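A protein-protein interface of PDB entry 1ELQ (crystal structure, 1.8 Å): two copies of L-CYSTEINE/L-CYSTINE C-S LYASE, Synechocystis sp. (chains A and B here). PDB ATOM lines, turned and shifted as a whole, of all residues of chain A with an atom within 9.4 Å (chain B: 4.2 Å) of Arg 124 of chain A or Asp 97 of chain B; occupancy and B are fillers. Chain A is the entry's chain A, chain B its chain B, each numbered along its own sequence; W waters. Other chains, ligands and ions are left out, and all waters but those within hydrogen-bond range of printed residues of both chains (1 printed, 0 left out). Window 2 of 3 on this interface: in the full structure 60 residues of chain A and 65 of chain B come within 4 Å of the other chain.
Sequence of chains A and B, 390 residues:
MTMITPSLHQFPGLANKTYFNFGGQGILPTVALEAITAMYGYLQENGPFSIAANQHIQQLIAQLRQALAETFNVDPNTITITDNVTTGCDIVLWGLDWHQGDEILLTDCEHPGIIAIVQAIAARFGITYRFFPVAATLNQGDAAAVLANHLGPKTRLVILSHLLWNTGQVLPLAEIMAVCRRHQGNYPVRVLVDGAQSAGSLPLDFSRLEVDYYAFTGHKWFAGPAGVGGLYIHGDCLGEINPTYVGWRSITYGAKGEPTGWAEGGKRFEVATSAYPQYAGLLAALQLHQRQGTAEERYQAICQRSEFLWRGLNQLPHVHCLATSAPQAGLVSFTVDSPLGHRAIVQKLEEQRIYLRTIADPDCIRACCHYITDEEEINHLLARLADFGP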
ATOM      1  N   LEU A  93      20.923   6.804  21.340  1.00  0.00           N
ATOM      2  CA  LEU A  93      20.549   5.867  22.384  1.00  0.00           C
ATOM      3  C   LEU A  93      19.614   4.739  21.929  1.00  0.00           C
ATOM      4  O   LEU A  93      19.832   3.566  22.277  1.00  0.00           O
ATOM      5  CB  LEU A  93      19.973   6.659  23.575  1.00  0.00           C
ATOM      6  CG  LEU A  93      21.046   7.585  24.210  1.00  0.00           C
ATOM      7  CD1 LEU A  93      20.421   8.444  25.304  1.00  0.00           C
ATOM      8  CD2 LEU A  93      22.191   6.724  24.824  1.00  0.00           C
ATOM      9  N   TRP A  94      18.589   5.062  21.139  1.00  0.00           N
ATOM     10  CA  TRP A  94      17.673   4.022  20.667  1.00  0.00           C
ATOM     11  C   TRP A  94      18.233   3.161  19.538  1.00  0.00           C
ATOM     12  O   TRP A  94      17.727   2.053  19.268  1.00  0.00           O
ATOM     13  CB  TRP A  94      16.359   4.637  20.195  1.00  0.00           C
ATOM     14  CG  TRP A  94      15.514   4.993  21.322  1.00  0.00           C
ATOM     15  CD1 TRP A  94      15.318   6.248  21.850  1.00  0.00           C
ATOM     16  CD2 TRP A  94      14.773   4.086  22.147  1.00  0.00           C
ATOM     17  NE1 TRP A  94      14.511   6.164  22.948  1.00  0.00           N
ATOM     18  CE2 TRP A  94      14.160   4.852  23.156  1.00  0.00           C
ATOM     19  CE3 TRP A  94      14.576   2.698  22.130  1.00  0.00           C
ATOM     20  CZ2 TRP A  94      13.348   4.277  24.152  1.00  0.00           C
ATOM     21  CZ3 TRP A  94      13.767   2.119  23.121  1.00  0.00           C
ATOM     22  CH2 TRP A  94      13.164   2.909  24.115  1.00  0.00           C
ATOM     23  N   TRP A  98      21.985  -2.522  22.047  1.00  0.00           N
ATOM     24  CA  TRP A  98      22.099  -2.905  23.468  1.00  0.00           C
ATOM     25  C   TRP A  98      21.785  -4.346  23.824  1.00  0.00           C
ATOM     26  O   TRP A  98      20.918  -4.971  23.210  1.00  0.00           O
ATOM     27  CB  TRP A  98      21.187  -2.050  24.362  1.00  0.00           C
ATOM     28  CG  TRP A  98      21.371  -0.571  24.216  1.00  0.00           C
ATOM     29  CD1 TRP A  98      20.564   0.309  23.525  1.00  0.00           C
ATOM     30  CD2 TRP A  98      22.470   0.200  24.716  1.00  0.00           C
ATOM     31  NE1 TRP A  98      21.112   1.574  23.566  1.00  0.00           N
ATOM     32  CE2 TRP A  98      22.276   1.535  24.288  1.00  0.00           C
ATOM     33  CE3 TRP A  98      23.605  -0.110  25.480  1.00  0.00           C
ATOM     34  CZ2 TRP A  98      23.175   2.553  24.598  1.00  0.00           C
ATOM     35  CZ3 TRP A  98      24.497   0.911  25.790  1.00  0.00           C
ATOM     36  CH2 TRP A  98      24.274   2.222  25.348  1.00  0.00           C
ATOM     37  N   HIS A  99      22.492  -4.846  24.842  1.00  0.00           N
ATOM     38  CA  HIS A  99      22.263  -6.191  25.380  1.00  0.00           C
ATOM     39  C   HIS A  99      22.158  -6.055  26.878  1.00  0.00           C
ATOM     40  O   HIS A  99      22.817  -5.195  27.467  1.00  0.00           O
ATOM     41  CB  HIS A  99      23.423  -7.125  25.089  1.00  0.00           C
ATOM     42  CG  HIS A  99      23.891  -7.075  23.680  1.00  0.00           C
ATOM     43  ND1 HIS A  99      25.155  -6.651  23.345  1.00  0.00           N
ATOM     44  CD2 HIS A  99      23.269  -7.380  22.519  1.00  0.00           C
ATOM     45  CE1 HIS A  99      25.294  -6.692  22.033  1.00  0.00           C
ATOM     46  NE2 HIS A  99      24.165  -7.131  21.508  1.00  0.00           N
ATOM     47  N   GLN A 100      21.343  -6.912  27.483  1.00  0.00           N
ATOM     48  CA  GLN A 100      21.157  -6.908  28.924  1.00  0.00           C
ATOM     49  C   GLN A 100      22.511  -6.894  29.611  1.00  0.00           C
ATOM     50  O   GLN A 100      23.408  -7.635  29.233  1.00  0.00           O
ATOM     51  CB  GLN A 100      20.382  -8.153  29.366  1.00  0.00           C
ATOM     52  CG  GLN A 100      18.950  -8.239  28.838  1.00  0.00           C
ATOM     53  CD  GLN A 100      18.257  -9.549  29.214  1.00  0.00           C
ATOM     54  OE1 GLN A 100      17.108  -9.790  28.834  1.00  0.00           O
ATOM     55  NE2 GLN A 100      18.960 -10.401  29.960  1.00  0.00           N
ATOM     56  N   ALA A 116      16.017  10.783  31.330  1.00  0.00           N
ATOM     57  CA  ALA A 116      14.755  10.108  31.002  1.00  0.00           C
ATOM     58  C   ALA A 116      14.916   9.112  29.856  1.00  0.00           C
ATOM     59  O   ALA A 116      14.343   8.029  29.913  1.00  0.00           O
ATOM     60  CB  ALA A 116      13.661  11.130  30.664  1.00  0.00           C
ATOM     61  N   ILE A 117      15.676   9.456  28.818  1.00  0.00           N
ATOM     62  CA  ILE A 117      15.876   8.507  27.728  1.00  0.00           C
ATOM     63  C   ILE A 117      16.634   7.285  28.284  1.00  0.00           C
ATOM     64  O   ILE A 117      16.245   6.139  28.030  1.00  0.00           O
ATOM     65  CB  ILE A 117      16.726   9.073  26.588  1.00  0.00           C
ATOM     66  CG1 ILE A 117      16.210  10.447  26.152  1.00  0.00           C
ATOM     67  CG2 ILE A 117      16.670   8.095  25.400  1.00  0.00           C
ATOM     68  CD1 ILE A 117      17.127  11.155  25.178  1.00  0.00           C
ATOM     69  N   VAL A 118      17.721   7.534  29.017  1.00  0.00           N
ATOM     70  CA  VAL A 118      18.507   6.450  29.598  1.00  0.00           C
ATOM     71  C   VAL A 118      17.668   5.450  30.397  1.00  0.00           C
ATOM     72  O   VAL A 118      17.859   4.245  30.258  1.00  0.00           O
ATOM     73  CB  VAL A 118      19.635   6.983  30.493  1.00  0.00           C
ATOM     74  CG1 VAL A 118      20.330   5.840  31.240  1.00  0.00           C
ATOM     75  CG2 VAL A 118      20.663   7.690  29.637  1.00  0.00           C
ATOM     76  N   GLN A 119      16.725   5.944  31.196  1.00  0.00           N
ATOM     77  CA  GLN A 119      15.878   5.074  32.019  1.00  0.00           C
ATOM     78  C   GLN A 119      14.918   4.278  31.132  1.00  0.00           C
ATOM     79  O   GLN A 119      14.584   3.133  31.448  1.00  0.00           O
ATOM     80  CB  GLN A 119      15.084   5.897  33.048  1.00  0.00           C
ATOM     81  CG  GLN A 119      15.972   6.785  33.914  1.00  0.00           C
ATOM     82  CD  GLN A 119      15.190   7.614  34.912  1.00  0.00           C
ATOM     83  OE1 GLN A 119      14.132   8.154  34.601  1.00  0.00           O
ATOM     84  NE2 GLN A 119      15.709   7.718  36.115  1.00  0.00           N
ATOM     85  N   ALA A 120      14.459   4.885  30.037  1.00  0.00           N
ATOM     86  CA  ALA A 120      13.579   4.175  29.114  1.00  0.00           C
ATOM     87  C   ALA A 120      14.401   3.079  28.429  1.00  0.00           C
ATOM     88  O   ALA A 120      13.917   1.969  28.242  1.00  0.00           O
ATOM     89  CB  ALA A 120      12.994   5.128  28.075  1.00  0.00           C
ATOM     90  N   ILE A 121      15.649   3.374  28.073  1.00  0.00           N
ATOM     91  CA  ILE A 121      16.493   2.358  27.431  1.00  0.00           C
ATOM     92  C   ILE A 121      16.780   1.237  28.434  1.00  0.00           C
ATOM     93  O   ILE A 121      16.699   0.057  28.102  1.00  0.00           O
ATOM     94  CB  ILE A 121      17.865   2.931  26.957  1.00  0.00           C
ATOM     95  CG1 ILE A 121      17.657   4.012  25.898  1.00  0.00           C
ATOM     96  CG2 ILE A 121      18.728   1.822  26.365  1.00  0.00           C
ATOM     97  CD1 ILE A 121      17.027   3.508  24.636  1.00  0.00           C
ATOM     98  N   ALA A 122      17.131   1.617  29.658  1.00  0.00           N
ATOM     99  CA  ALA A 122      17.423   0.648  30.693  1.00  0.00           C
ATOM    100  C   ALA A 122      16.214  -0.283  30.769  1.00  0.00           C
ATOM    101  O   ALA A 122      16.366  -1.488  30.723  1.00  0.00           O
ATOM    102  CB  ALA A 122      17.650   1.349  32.018  1.00  0.00           C
ATOM    103  N   ALA A 123      15.018   0.289  30.859  1.00  0.00           N
ATOM    104  CA  ALA A 123      13.778  -0.487  30.924  1.00  0.00           C
ATOM    105  C   ALA A 123      13.501  -1.365  29.685  1.00  0.00           C
ATOM    106  O   ALA A 123      12.943  -2.461  29.790  1.00  0.00           O
ATOM    107  CB  ALA A 123      12.621   0.449  31.136  1.00  0.00           C
ATOM    108  N   ARG A 124      13.885  -0.886  28.507  1.00  0.00           N
ATOM    109  CA  ARG A 124      13.627  -1.619  27.275  1.00  0.00           C
ATOM    110  C   ARG A 124      14.644  -2.715  26.925  1.00  0.00           C
ATOM    111  O   ARG A 124      14.273  -3.798  26.466  1.00  0.00           O
ATOM    112  CB  ARG A 124      13.550  -0.634  26.105  1.00  0.00           C
ATOM    113  CG  ARG A 124      12.833  -1.170  24.898  1.00  0.00           C
ATOM    114  CD  ARG A 124      11.333  -1.006  25.103  1.00  0.00           C
ATOM    115  NE  ARG A 124      10.569  -1.872  24.211  1.00  0.00           N
ATOM    116  CZ  ARG A 124       9.644  -1.435  23.363  1.00  0.00           C
ATOM    117  NH1 ARG A 124       9.376  -0.131  23.297  1.00  0.00           N
ATOM    118  NH2 ARG A 124       8.983  -2.303  22.590  1.00  0.00           N
ATOM    119  N   PHE A 125      15.924  -2.434  27.121  1.00  0.00           N
ATOM    120  CA  PHE A 125      16.959  -3.389  26.778  1.00  0.00           C
ATOM    121  C   PHE A 125      17.622  -4.083  27.959  1.00  0.00           C
ATOM    122  O   PHE A 125      18.502  -4.916  27.776  1.00  0.00           O
ATOM    123  CB  PHE A 125      18.057  -2.700  25.967  1.00  0.00           C
ATOM    124  CG  PHE A 125      17.580  -2.070  24.690  1.00  0.00           C
ATOM    125  CD1 PHE A 125      17.121  -0.763  24.676  1.00  0.00           C
ATOM    126  CD2 PHE A 125      17.661  -2.767  23.486  1.00  0.00           C
ATOM    127  CE1 PHE A 125      16.758  -0.153  23.490  1.00  0.00           C
ATOM    128  CE2 PHE A 125      17.299  -2.163  22.284  1.00  0.00           C
ATOM    129  CZ  PHE A 125      16.849  -0.855  22.285  1.00  0.00           C
ATOM    130  N   GLY A 126      17.214  -3.743  29.170  1.00  0.00           N
ATOM    131  CA  GLY A 126      17.836  -4.370  30.321  1.00  0.00           C
ATOM    132  C   GLY A 126      19.266  -3.899  30.525  1.00  0.00           C
ATOM    133  O   GLY A 126      20.116  -4.671  30.976  1.00  0.00           O
ATOM    134  N   ILE A 127      19.575  -2.654  30.162  1.00  0.00           N
ATOM    135  CA  ILE A 127      20.934  -2.171  30.406  1.00  0.00           C
ATOM    136  C   ILE A 127      20.884  -1.494  31.777  1.00  0.00           C
ATOM    137  O   ILE A 127      19.808  -1.336  32.357  1.00  0.00           O
ATOM    138  CB  ILE A 127      21.429  -1.141  29.335  1.00  0.00           C
ATOM    139  CG1 ILE A 127      20.491   0.069  29.272  1.00  0.00           C
ATOM    140  CG2 ILE A 127      21.543  -1.791  27.979  1.00  0.00           C
ATOM    141  CD1 ILE A 127      20.798   1.153  30.285  1.00  0.00           C
ATOM    142  N   THR A 128      22.042  -1.120  32.307  1.00  0.00           N
ATOM    143  CA  THR A 128      22.105  -0.434  33.600  1.00  0.00           C
ATOM    144  C   THR A 128      22.830   0.921  33.434  1.00  0.00           C
ATOM    145  O   THR A 128      23.605   1.105  32.478  1.00  0.00           O
ATOM    146  CB  THR A 128      22.890  -1.275  34.649  1.00  0.00           C
ATOM    147  OG1 THR A 128      24.274  -1.369  34.268  1.00  0.00           O
ATOM    148  CG2 THR A 128      22.296  -2.686  34.748  1.00  0.00           C
ATOM    149  N   THR A 244      15.728   4.470  14.041  1.00  0.00           N
ATOM    150  CA  THR A 244      14.606   4.074  14.877  1.00  0.00           C
ATOM    151  C   THR A 244      13.406   4.842  14.381  1.00  0.00           C
ATOM    152  O   THR A 244      12.609   4.308  13.608  1.00  0.00           O
ATOM    153  CB  THR A 244      14.858   4.381  16.372  1.00  0.00           C
ATOM    154  OG1 THR A 244      15.976   3.610  16.845  1.00  0.00           O
ATOM    155  CG2 THR A 244      13.625   3.999  17.196  1.00  0.00           C
ATOM    156  N   TYR A 245      13.243   6.094  14.797  1.00  0.00           N
ATOM    157  CA  TYR A 245      12.108   6.826  14.256  1.00  0.00           C
ATOM    158  C   TYR A 245      12.457   7.165  12.818  1.00  0.00           C
ATOM    159  O   TYR A 245      13.410   7.888  12.562  1.00  0.00           O
ATOM    160  CB  TYR A 245      11.833   8.121  15.023  1.00  0.00           C
ATOM    161  CG  TYR A 245      10.880   7.994  16.211  1.00  0.00           C
ATOM    162  CD1 TYR A 245      10.251   9.127  16.739  1.00  0.00           C
ATOM    163  CD2 TYR A 245      10.727   6.775  16.898  1.00  0.00           C
ATOM    164  CE1 TYR A 245       9.505   9.061  17.921  1.00  0.00           C
ATOM    165  CE2 TYR A 245       9.993   6.703  18.081  1.00  0.00           C
ATOM    166  CZ  TYR A 245       9.385   7.848  18.585  1.00  0.00           C
ATOM    167  OH  TYR A 245       8.641   7.786  19.746  1.00  0.00           O
ATOM    168  N   TRP B  94       6.800   1.927  17.673  1.00  0.00           N
ATOM    169  CA  TRP B  94       7.948   1.649  18.540  1.00  0.00           C
ATOM    170  C   TRP B  94       7.593   1.473  20.018  1.00  0.00           C
ATOM    171  O   TRP B  94       8.375   0.917  20.783  1.00  0.00           O
ATOM    172  CB  TRP B  94       8.967   2.759  18.427  1.00  0.00           C
ATOM    173  CG  TRP B  94       9.699   2.703  17.178  1.00  0.00           C
ATOM    174  CD1 TRP B  94       9.532   3.505  16.090  1.00  0.00           C
ATOM    175  CD2 TRP B  94      10.753   1.793  16.855  1.00  0.00           C
ATOM    176  NE1 TRP B  94      10.422   3.153  15.113  1.00  0.00           N
ATOM    177  CE2 TRP B  94      11.185   2.107  15.554  1.00  0.00           C
ATOM    178  CE3 TRP B  94      11.373   0.737  17.545  1.00  0.00           C
ATOM    179  CZ2 TRP B  94      12.213   1.412  14.918  1.00  0.00           C
ATOM    180  CZ3 TRP B  94      12.393   0.042  16.913  1.00  0.00           C
ATOM    181  CH2 TRP B  94      12.804   0.384  15.611  1.00  0.00           C
ATOM    182  N   GLY B  95       6.416   1.962  20.402  1.00  0.00           N
ATOM    183  CA  GLY B  95       5.976   1.879  21.778  1.00  0.00           C
ATOM    184  C   GLY B  95       5.442   0.499  22.146  1.00  0.00           C
ATOM    185  O   GLY B  95       5.521   0.094  23.298  1.00  0.00           O
ATOM    186  N   LEU B  96       4.895  -0.221  21.178  1.00  0.00           N
ATOM    187  CA  LEU B  96       4.362  -1.547  21.447  1.00  0.00           C
ATOM    188  C   LEU B  96       5.429  -2.568  21.841  1.00  0.00           C
ATOM    189  O   LEU B  96       6.537  -2.578  21.328  1.00  0.00           O
ATOM    190  CB  LEU B  96       3.595  -2.033  20.229  1.00  0.00           C
ATOM    191  CG  LEU B  96       2.293  -1.264  20.094  1.00  0.00           C
ATOM    192  CD1 LEU B  96       1.774  -1.389  18.685  1.00  0.00           C
ATOM    193  CD2 LEU B  96       1.303  -1.785  21.127  1.00  0.00           C
ATOM    194  N   ASP B  97       5.072  -3.432  22.780  1.00  0.00           N
ATOM    195  CA  ASP B  97       5.986  -4.461  23.261  1.00  0.00           C
ATOM    196  C   ASP B  97       5.999  -5.644  22.283  1.00  0.00           C
ATOM    197  O   ASP B  97       5.371  -6.678  22.558  1.00  0.00           O
ATOM    198  CB  ASP B  97       5.502  -4.922  24.635  1.00  0.00           C
ATOM    199  CG  ASP B  97       6.442  -5.885  25.280  1.00  0.00           C
ATOM    200  OD1 ASP B  97       5.926  -6.788  25.980  1.00  0.00           O
ATOM    201  OD2 ASP B  97       7.677  -5.730  25.087  1.00  0.00           O
ATOM    202  N   TRP B  98       6.701  -5.492  21.153  1.00  0.00           N
ATOM    203  CA  TRP B  98       6.779  -6.534  20.112  1.00  0.00           C
ATOM    204  C   TRP B  98       7.552  -7.802  20.476  1.00  0.00           C
ATOM    205  O   TRP B  98       8.676  -7.726  20.992  1.00  0.00           O
ATOM    206  CB  TRP B  98       7.420  -5.982  18.832  1.00  0.00           C
ATOM    207  CG  TRP B  98       6.623  -4.903  18.155  1.00  0.00           C
ATOM    208  CD1 TRP B  98       6.939  -3.580  18.093  1.00  0.00           C
ATOM    209  CD2 TRP B  98       5.333  -5.041  17.529  1.00  0.00           C
ATOM    210  NE1 TRP B  98       5.931  -2.887  17.481  1.00  0.00           N
ATOM    211  CE2 TRP B  98       4.931  -3.754  17.122  1.00  0.00           C
ATOM    212  CE3 TRP B  98       4.481  -6.124  17.278  1.00  0.00           C
ATOM    213  CZ2 TRP B  98       3.708  -3.513  16.476  1.00  0.00           C
ATOM    214  CZ3 TRP B  98       3.262  -5.891  16.634  1.00  0.00           C
ATOM    215  CH2 TRP B  98       2.885  -4.596  16.240  1.00  0.00           C
ATOM    216  N   HIS B  99       6.954  -8.957  20.180  1.00  0.00           N
ATOM    217  CA  HIS B  99       7.619 -10.243  20.409  1.00  0.00           C
ATOM    218  C   HIS B  99       7.754 -10.896  19.038  1.00  0.00           C
ATOM    219  O   HIS B  99       6.826 -10.816  18.220  1.00  0.00           O
ATOM    220  CB  HIS B  99       6.801 -11.148  21.338  1.00  0.00           C
ATOM    221  CG  HIS B  99       6.386 -10.479  22.609  1.00  0.00           C
ATOM    222  ND1 HIS B  99       5.063 -10.281  22.950  1.00  0.00           N
ATOM    223  CD2 HIS B  99       7.118  -9.909  23.595  1.00  0.00           C
ATOM    224  CE1 HIS B  99       4.999  -9.618  24.090  1.00  0.00           C
ATOM    225  NE2 HIS B  99       6.232  -9.377  24.501  1.00  0.00           N
ATOM    226  N   PHE B 125      12.490  -6.440  16.187  1.00  0.00           N
ATOM    227  CA  PHE B 125      11.906  -7.406  17.108  1.00  0.00           C
ATOM    228  C   PHE B 125      11.545  -8.772  16.503  1.00  0.00           C
ATOM    229  O   PHE B 125      10.958  -9.618  17.182  1.00  0.00           O
ATOM    230  CB  PHE B 125      10.666  -6.794  17.776  1.00  0.00           C
ATOM    231  CG  PHE B 125      10.936  -5.485  18.457  1.00  0.00           C
ATOM    232  CD1 PHE B 125      10.632  -4.280  17.827  1.00  0.00           C
ATOM    233  CD2 PHE B 125      11.536  -5.452  19.717  1.00  0.00           C
ATOM    234  CE1 PHE B 125      10.925  -3.056  18.441  1.00  0.00           C
ATOM    235  CE2 PHE B 125      11.832  -4.233  20.337  1.00  0.00           C
ATOM    236  CZ  PHE B 125      11.527  -3.034  19.698  1.00  0.00           C
ATOM    237  N   ARG B 156      -1.429  -8.741  15.471  1.00  0.00           N
ATOM    238  CA  ARG B 156      -1.507  -7.899  16.653  1.00  0.00           C
ATOM    239  C   ARG B 156      -1.941  -6.479  16.289  1.00  0.00           C
ATOM    240  O   ARG B 156      -2.674  -5.816  17.037  1.00  0.00           O
ATOM    241  CB  ARG B 156      -0.137  -7.863  17.333  1.00  0.00           C
ATOM    242  CG  ARG B 156      -0.122  -7.151  18.690  1.00  0.00           C
ATOM    243  CD  ARG B 156       1.159  -7.450  19.452  1.00  0.00           C
ATOM    244  NE  ARG B 156       1.164  -6.844  20.785  1.00  0.00           N
ATOM    245  CZ  ARG B 156       2.114  -7.052  21.699  1.00  0.00           C
ATOM    246  NH1 ARG B 156       3.134  -7.859  21.415  1.00  0.00           N
ATOM    247  NH2 ARG B 156       2.047  -6.454  22.894  1.00  0.00           N
HETATM  248  O   HOH W   1       9.807  -5.575  22.461  1.00  0.00           O
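O of Trp 94 of chain A is in hydrogen-bond range of OG1 of Thr 244 of chain A. The side-chain carboxylate (OD1) of Asp 97 of chain B lies within hydrogen-bond range of a ring nitrogen (NE2) of His 99 of chain B, 3.0 Å away. The backbone carbonyl oxygen of Asp 97 of chain B lies within hydrogen-bond range of the guanidinium group of Arg 156 of chain B (2.8 Å).
NH1 of Arg 124 of chain A touches O of Gly 95 of chain B (3.9 Å). Arg 124 of chain A touches Asp 97 of chain B. Arg 124 of chain A touches Phe 125 of chain B. Trp 94 of chain B touches Tyr 245 of chain A (CD1 to CD2, 3.6 Å).
O of Thr 244 of chain A is in hydrogen-bond range of NE1 of Trp 94 of chain B, 2.9 Å away. The backbone carbonyl oxygen of Trp 94 of chain B is in hydrogen-bond range of the guanidinium group of Arg 124 of chain A (2.9 Å). The guanidinium group of Arg 124 of chain A is in hydrogen-bond range of the backbone carbonyl oxygen of Leu 96 of chain B.
Positions printed for both chains: 94, 98, 99 and 125.
Arg 124 of chain A touches five residues of chain B. Of chain A, only Arg 124 (3.8 Å) comes within 4 Å of Asp 97 of chain B. Gly 95 of chain B touches one residue of chain A. Of the printed residues of chain A, Phe 125 of chain B touches Arg 124. Of the printed residues of chain B, Tyr 245 of chain A touches Trp 94 (3.6 Å). Printed residues of chain A within 4 Å of Trp 94 of chain B: Arg 124 (2.9 Å), Thr 244 (2.9 Å) and Tyr 245 (3.6 Å). The nearest residue of chain A that does not touch Asp 97 of chain B is Ala 123 of chain A (7.8 Å).
Water W1 lies within hydrogen-bond range of the backbone carbonyl oxygen of Trp 98 of chain B, the guanidinium group of Arg 124 of chain A and the side-chain carboxylate of Asp 97 of chain B.
Of the 8 printed residues of chain B, 5 touch a printed residue of chain A. Printed residues of chain B that touch a printed residue of chain A: Trp 94, Gly 95, Leu 96, Asp 97 and Phe 125. Hydrophobic or aromatic side chains of chain A that line the printed part of chain B: Tyr 245. Among the printed residues, 7 pairs touch across the chains. Among the printed residues, no Asp or Glu carboxylate lies within 4 Å of a Lys or Arg side-chain nitrogen of the other chain.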
